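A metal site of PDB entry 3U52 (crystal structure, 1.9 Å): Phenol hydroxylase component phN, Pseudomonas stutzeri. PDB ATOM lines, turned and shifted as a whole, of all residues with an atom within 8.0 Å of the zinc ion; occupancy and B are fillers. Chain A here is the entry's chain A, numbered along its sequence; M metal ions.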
ATOM      1  N   TRP A 267      12.605 -11.319 -16.472  1.00  0.00           N
ATOM      2  CA  TRP A 267      12.724 -12.036 -15.215  1.00  0.00           C
ATOM      3  C   TRP A 267      11.377 -12.668 -14.797  1.00  0.00           C
ATOM      4  O   TRP A 267      11.317 -13.833 -14.453  1.00  0.00           O
ATOM      5  CB  TRP A 267      13.375 -11.207 -14.099  1.00  0.00           C
ATOM      6  CG  TRP A 267      13.612 -12.105 -12.910  1.00  0.00           C
ATOM      7  CD1 TRP A 267      12.842 -12.205 -11.789  1.00  0.00           C
ATOM      8  CD2 TRP A 267      14.690 -13.034 -12.735  1.00  0.00           C
ATOM      9  NE1 TRP A 267      13.355 -13.152 -10.953  1.00  0.00           N
ATOM     10  CE2 TRP A 267      14.486 -13.683 -11.515  1.00  0.00           C
ATOM     11  CE3 TRP A 267      15.797 -13.393 -13.516  1.00  0.00           C
ATOM     12  CZ2 TRP A 267      15.374 -14.683 -11.017  1.00  0.00           C
ATOM     13  CZ3 TRP A 267      16.683 -14.371 -13.021  1.00  0.00           C
ATOM     14  CH2 TRP A 267      16.461 -15.004 -11.799  1.00  0.00           C
ATOM     15  N   ARG A 268      10.274 -11.916 -14.921  1.00  0.00           N
ATOM     16  CA  ARG A 268       8.941 -12.504 -14.732  1.00  0.00           C
ATOM     17  C   ARG A 268       8.616 -13.668 -15.719  1.00  0.00           C
ATOM     18  O   ARG A 268       8.004 -14.667 -15.328  1.00  0.00           O
ATOM     19  CB  ARG A 268       7.848 -11.410 -14.821  1.00  0.00           C
ATOM     20  CG  ARG A 268       7.843 -10.485 -13.573  1.00  0.00           C
ATOM     21  CD  ARG A 268       6.370 -10.112 -13.137  1.00  0.00           C
ATOM     22  NE  ARG A 268       5.681 -11.285 -12.587  1.00  0.00           N
ATOM     23  CZ  ARG A 268       4.634 -11.233 -11.786  1.00  0.00           C
ATOM     24  NH1 ARG A 268       4.119 -10.075 -11.441  1.00  0.00           N
ATOM     25  NH2 ARG A 268       4.078 -12.353 -11.340  1.00  0.00           N
ATOM     26  N   ARG A 271      10.511 -16.792 -14.607  1.00  0.00           N
ATOM     27  CA  ARG A 271       9.858 -17.452 -13.471  1.00  0.00           C
ATOM     28  C   ARG A 271       8.596 -18.165 -13.943  1.00  0.00           C
ATOM     29  O   ARG A 271       8.321 -19.288 -13.539  1.00  0.00           O
ATOM     30  CB  ARG A 271       9.597 -16.452 -12.317  1.00  0.00           C
ATOM     31  CG  ARG A 271      10.924 -16.120 -11.585  1.00  0.00           C
ATOM     32  CD  ARG A 271      11.442 -17.398 -10.922  1.00  0.00           C
ATOM     33  NE  ARG A 271      12.441 -17.113  -9.858  1.00  0.00           N
ATOM     34  CZ  ARG A 271      13.634 -17.687  -9.776  1.00  0.00           C
ATOM     35  NH1 ARG A 271      14.065 -18.561 -10.675  1.00  0.00           N
ATOM     36  NH2 ARG A 271      14.429 -17.359  -8.769  1.00  0.00           N
ATOM     37  N   LEU A 398       6.077 -17.830  -0.014  1.00  0.00           N
ATOM     38  CA  LEU A 398       5.929 -17.479  -1.403  1.00  0.00           C
ATOM     39  C   LEU A 398       6.688 -16.183  -1.668  1.00  0.00           C
ATOM     40  O   LEU A 398       6.757 -15.305  -0.771  1.00  0.00           O
ATOM     41  CB  LEU A 398       4.438 -17.264  -1.737  1.00  0.00           C
ATOM     42  CG  LEU A 398       3.477 -18.439  -1.564  1.00  0.00           C
ATOM     43  CD1 LEU A 398       2.114 -18.047  -2.133  1.00  0.00           C
ATOM     44  CD2 LEU A 398       4.035 -19.685  -2.274  1.00  0.00           C
ATOM     45  N   CYS A 399       7.225 -16.026  -2.894  1.00  0.00           N
ATOM     46  CA  CYS A 399       7.831 -14.768  -3.310  1.00  0.00           C
ATOM     47  C   CYS A 399       6.761 -13.686  -3.455  1.00  0.00           C
ATOM     48  O   CYS A 399       5.750 -13.911  -4.093  1.00  0.00           O
ATOM     49  CB  CYS A 399       8.521 -14.922  -4.659  1.00  0.00           C
ATOM     50  SG  CYS A 399       9.385 -13.469  -5.292  1.00  0.00           S
ATOM     51  N   GLN A 400       7.049 -12.474  -2.944  1.00  0.00           N
ATOM     52  CA  GLN A 400       6.118 -11.362  -3.011  1.00  0.00           C
ATOM     53  C   GLN A 400       5.803 -10.955  -4.495  1.00  0.00           C
ATOM     54  O   GLN A 400       4.755 -10.340  -4.787  1.00  0.00           O
ATOM     55  CB  GLN A 400       6.686 -10.146  -2.253  1.00  0.00           C
ATOM     56  CG  GLN A 400       5.657  -8.933  -2.094  1.00  0.00           C
ATOM     57  CD  GLN A 400       4.449  -9.329  -1.273  1.00  0.00           C
ATOM     58  OE1 GLN A 400       3.275  -8.928  -1.551  1.00  0.00           O
ATOM     59  NE2 GLN A 400       4.692 -10.050  -0.244  1.00  0.00           N
ATOM     60  N   VAL A 401       6.679 -11.306  -5.423  1.00  0.00           N
ATOM     61  CA  VAL A 401       6.540 -10.797  -6.826  1.00  0.00           C
ATOM     62  C   VAL A 401       6.037 -11.935  -7.722  1.00  0.00           C
ATOM     63  O   VAL A 401       4.938 -11.845  -8.272  1.00  0.00           O
ATOM     64  CB  VAL A 401       7.846 -10.137  -7.376  1.00  0.00           C
ATOM     65  CG1 VAL A 401       7.751  -9.864  -8.881  1.00  0.00           C
ATOM     66  CG2 VAL A 401       8.199  -8.821  -6.582  1.00  0.00           C
ATOM     67  N   CYS A 402       6.775 -13.036  -7.828  1.00  0.00           N
ATOM     68  CA  CYS A 402       6.439 -14.055  -8.848  1.00  0.00           C
ATOM     69  C   CYS A 402       5.482 -15.048  -8.259  1.00  0.00           C
ATOM     70  O   CYS A 402       4.814 -15.765  -9.020  1.00  0.00           O
ATOM     71  CB  CYS A 402       7.722 -14.740  -9.430  1.00  0.00           C
ATOM     72  SG  CYS A 402       8.617 -15.810  -8.270  1.00  0.00           S
ATOM     73  N   GLN A 403       5.344 -15.002  -6.914  1.00  0.00           N
ATOM     74  CA  GLN A 403       4.525 -15.919  -6.094  1.00  0.00           C
ATOM     75  C   GLN A 403       4.819 -17.401  -6.131  1.00  0.00           C
ATOM     76  O   GLN A 403       4.045 -18.160  -5.607  1.00  0.00           O
ATOM     77  CB  GLN A 403       3.016 -15.686  -6.259  1.00  0.00           C
ATOM     78  CG  GLN A 403       2.724 -14.138  -6.245  1.00  0.00           C
ATOM     79  CD  GLN A 403       1.279 -13.814  -6.373  1.00  0.00           C
ATOM     80  OE1 GLN A 403       0.420 -14.689  -6.241  1.00  0.00           O
ATOM     81  NE2 GLN A 403       0.981 -12.540  -6.629  1.00  0.00           N
ATOM     82  N   ILE A 404       5.960 -17.801  -6.660  1.00  0.00           N
ATOM     83  CA  ILE A 404       6.378 -19.201  -6.575  1.00  0.00           C
ATOM     84  C   ILE A 404       6.896 -19.377  -5.102  1.00  0.00           C
ATOM     85  O   ILE A 404       7.469 -18.445  -4.552  1.00  0.00           O
ATOM     86  CB  ILE A 404       7.500 -19.483  -7.608  1.00  0.00           C
ATOM     87  CG1 ILE A 404       6.989 -19.188  -9.027  1.00  0.00           C
ATOM     88  CG2 ILE A 404       7.979 -20.995  -7.543  1.00  0.00           C
ATOM     89  CD1 ILE A 404       7.993 -19.406 -10.176  1.00  0.00           C
ATOM     90  N   PRO A 405       6.694 -20.550  -4.482  1.00  0.00           N
ATOM     91  CA  PRO A 405       7.383 -20.778  -3.224  1.00  0.00           C
ATOM     92  C   PRO A 405       8.869 -20.457  -3.383  1.00  0.00           C
ATOM     93  O   PRO A 405       9.430 -20.622  -4.460  1.00  0.00           O
ATOM     94  CB  PRO A 405       7.231 -22.261  -2.989  1.00  0.00           C
ATOM     95  CG  PRO A 405       6.062 -22.672  -3.674  1.00  0.00           C
ATOM     96  CD  PRO A 405       5.859 -21.703  -4.849  1.00  0.00           C
ATOM     97  N   THR A 406       9.525 -20.069  -2.312  1.00  0.00           N
ATOM     98  CA  THR A 406      10.944 -19.703  -2.395  1.00  0.00           C
ATOM     99  C   THR A 406      11.834 -20.963  -2.386  1.00  0.00           C
ATOM    100  O   THR A 406      12.449 -21.295  -1.393  1.00  0.00           O
ATOM    101  CB  THR A 406      11.310 -18.694  -1.280  1.00  0.00           C
ATOM    102  OG1 THR A 406      10.749 -19.142  -0.043  1.00  0.00           O
ATOM    103  CG2 THR A 406      10.627 -17.416  -1.568  1.00  0.00           C
ATOM    104  N   PHE A 408      14.208 -21.769  -4.924  1.00  0.00           N
ATOM    105  CA  PHE A 408      15.335 -21.642  -5.839  1.00  0.00           C
ATOM    106  C   PHE A 408      16.620 -21.384  -5.080  1.00  0.00           C
ATOM    107  O   PHE A 408      16.598 -20.780  -4.026  1.00  0.00           O
ATOM    108  CB  PHE A 408      15.066 -20.475  -6.799  1.00  0.00           C
ATOM    109  CG  PHE A 408      13.828 -20.660  -7.594  1.00  0.00           C
ATOM    110  CD1 PHE A 408      12.713 -19.872  -7.358  1.00  0.00           C
ATOM    111  CD2 PHE A 408      13.766 -21.638  -8.561  1.00  0.00           C
ATOM    112  CE1 PHE A 408      11.504 -20.073  -8.105  1.00  0.00           C
ATOM    113  CE2 PHE A 408      12.599 -21.840  -9.321  1.00  0.00           C
ATOM    114  CZ  PHE A 408      11.476 -21.062  -9.077  1.00  0.00           C
ATOM    115  N   HIS A 430       9.395 -10.640   1.335  1.00  0.00           N
ATOM    116  CA  HIS A 430      10.364 -11.692   0.973  1.00  0.00           C
ATOM    117  C   HIS A 430      10.269 -12.046  -0.527  1.00  0.00           C
ATOM    118  O   HIS A 430       9.172 -12.002  -1.141  1.00  0.00           O
ATOM    119  CB  HIS A 430      10.104 -12.955   1.802  1.00  0.00           C
ATOM    120  CG  HIS A 430      10.143 -12.699   3.290  1.00  0.00           C
ATOM    121  ND1 HIS A 430      11.268 -12.939   4.049  1.00  0.00           N
ATOM    122  CD2 HIS A 430       9.239 -12.126   4.117  1.00  0.00           C
ATOM    123  CE1 HIS A 430      11.031 -12.573   5.298  1.00  0.00           C
ATOM    124  NE2 HIS A 430       9.809 -12.069   5.360  1.00  0.00           N
ATOM    125  N   PHE A 431      11.414 -12.478  -1.064  1.00  0.00           N
ATOM    126  CA  PHE A 431      11.603 -12.763  -2.507  1.00  0.00           C
ATOM    127  C   PHE A 431      12.387 -14.058  -2.715  1.00  0.00           C
ATOM    128  O   PHE A 431      13.148 -14.467  -1.837  1.00  0.00           O
ATOM    129  CB  PHE A 431      12.329 -11.579  -3.173  1.00  0.00           C
ATOM    130  CG  PHE A 431      11.733 -10.269  -2.808  1.00  0.00           C
ATOM    131  CD1 PHE A 431      10.538  -9.835  -3.397  1.00  0.00           C
ATOM    132  CD2 PHE A 431      12.270  -9.508  -1.778  1.00  0.00           C
ATOM    133  CE1 PHE A 431       9.922  -8.630  -2.981  1.00  0.00           C
ATOM    134  CE2 PHE A 431      11.683  -8.258  -1.383  1.00  0.00           C
ATOM    135  CZ  PHE A 431      10.508  -7.853  -1.961  1.00  0.00           C
ATOM    136  N   CYS A 432      12.240 -14.664  -3.907  1.00  0.00           N
ATOM    137  CA  CYS A 432      12.983 -15.889  -4.238  1.00  0.00           C
ATOM    138  C   CYS A 432      14.409 -15.596  -4.792  1.00  0.00           C
ATOM    139  O   CYS A 432      15.198 -16.549  -4.957  1.00  0.00           O
ATOM    140  CB  CYS A 432      12.200 -16.649  -5.298  1.00  0.00           C
ATOM    141  SG  CYS A 432      12.075 -15.702  -6.858  1.00  0.00           S
ATOM    142  N   SER A 433      14.716 -14.338  -5.086  1.00  0.00           N
ATOM    143  CA  SER A 433      15.909 -13.965  -5.847  1.00  0.00           C
ATOM    144  C   SER A 433      16.127 -12.456  -5.861  1.00  0.00           C
ATOM    145  O   SER A 433      15.237 -11.695  -5.504  1.00  0.00           O
ATOM    146  CB  SER A 433      15.721 -14.378  -7.300  1.00  0.00           C
ATOM    147  OG  SER A 433      14.513 -13.751  -7.782  1.00  0.00           O
ATOM    148  N   ASP A 434      17.304 -12.037  -6.342  1.00  0.00           N
ATOM    149  CA  ASP A 434      17.614 -10.645  -6.607  1.00  0.00           C
ATOM    150  C   ASP A 434      16.712 -10.131  -7.714  1.00  0.00           C
ATOM    151  O   ASP A 434      16.366  -8.978  -7.710  1.00  0.00           O
ATOM    152  CB  ASP A 434      19.071 -10.464  -7.030  1.00  0.00           C
ATOM    153  CG  ASP A 434      20.063 -10.695  -5.881  1.00  0.00           C
ATOM    154  OD1 ASP A 434      19.865 -10.157  -4.765  1.00  0.00           O
ATOM    155  OD2 ASP A 434      21.052 -11.409  -6.114  1.00  0.00           O
ATOM    156  N   GLY A 435      16.360 -10.961  -8.673  1.00  0.00           N
ATOM    157  CA  GLY A 435      15.620 -10.453  -9.823  1.00  0.00           C
ATOM    158  C   GLY A 435      14.241  -9.950  -9.403  1.00  0.00           C
ATOM    159  O   GLY A 435      13.817  -8.889  -9.833  1.00  0.00           O
ATOM    160  N   CYS A 436      13.578 -10.712  -8.535  1.00  0.00           N
ATOM    161  CA  CYS A 436      12.252 -10.357  -8.005  1.00  0.00           C
ATOM    162  C   CYS A 436      12.378  -9.214  -6.991  1.00  0.00           C
ATOM    163  O   CYS A 436      11.581  -8.316  -6.973  1.00  0.00           O
ATOM    164  CB  CYS A 436      11.607 -11.573  -7.387  1.00  0.00           C
ATOM    165  SG  CYS A 436      10.832 -12.725  -8.649  1.00  0.00           S
ATOM    166  N   CYS A 437      13.423  -9.242  -6.192  1.00  0.00           N
ATOM    167  CA  CYS A 437      13.701  -8.116  -5.282  1.00  0.00           C
ATOM    168  C   CYS A 437      13.788  -6.795  -6.031  1.00  0.00           C
ATOM    169  O   CYS A 437      13.159  -5.818  -5.623  1.00  0.00           O
ATOM    170  CB  CYS A 437      14.977  -8.406  -4.437  1.00  0.00           C
ATOM    171  SG  CYS A 437      15.147  -7.182  -3.071  1.00  0.00           S
ATOM    172  N   ILE A 439      12.563  -5.903  -8.981  1.00  0.00           N
ATOM    173  CA  ILE A 439      11.273  -5.548  -9.535  1.00  0.00           C
ATOM    174  C   ILE A 439      10.427  -4.894  -8.383  1.00  0.00           C
ATOM    175  O   ILE A 439       9.771  -3.839  -8.570  1.00  0.00           O
ATOM    176  CB  ILE A 439      10.529  -6.826 -10.086  1.00  0.00           C
ATOM    177  CG1 ILE A 439      11.238  -7.348 -11.333  1.00  0.00           C
ATOM    178  CG2 ILE A 439       9.029  -6.530 -10.362  1.00  0.00           C
ATOM    179  CD1 ILE A 439      10.823  -8.709 -11.754  1.00  0.00           C
HETATM  180 ZN    ZN M   1      10.149 -14.424  -7.339  1.00  0.00          ZN
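Within 4 Å of the zinc ion: Cys 399, Cys 402, Cys 432 and Cys 436. The nearest printed residue that does not touch the zinc ion is Arg 271 (4.3 Å).
NE1 of Trp 267 sits close to SG of Cys 436, 3.4 Å away. N of Cys 399 is in hydrogen-bond range of O of Ile 404, at 2.9 Å. N of Ile 404 lies close to SG of Cys 402 (3.7 Å). N of Val 401 sits close to SG of Cys 399 (3.5 Å). The backbone NH of Cys 436 sits at hydrogen-bond distance from the side-chain hydroxyl of Ser 433 (3.3 Å). SG of Cys 432 lies close to NE of Arg 271, at 3.3 Å. OG of Ser 433 sits close to SG of Cys 432 (3.3 Å).
SG of Cys 436 binds the zinc ion, 2.3 Å away. The side-chain sulfur (SG) of Cys 402 is bound to the zinc ion. The side-chain sulfur (SG) of Cys 432 binds the zinc ion, at 2.4 Å. The zinc ion is bound by the side-chain sulfur (SG) of Cys 399, at 2.4 Å.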
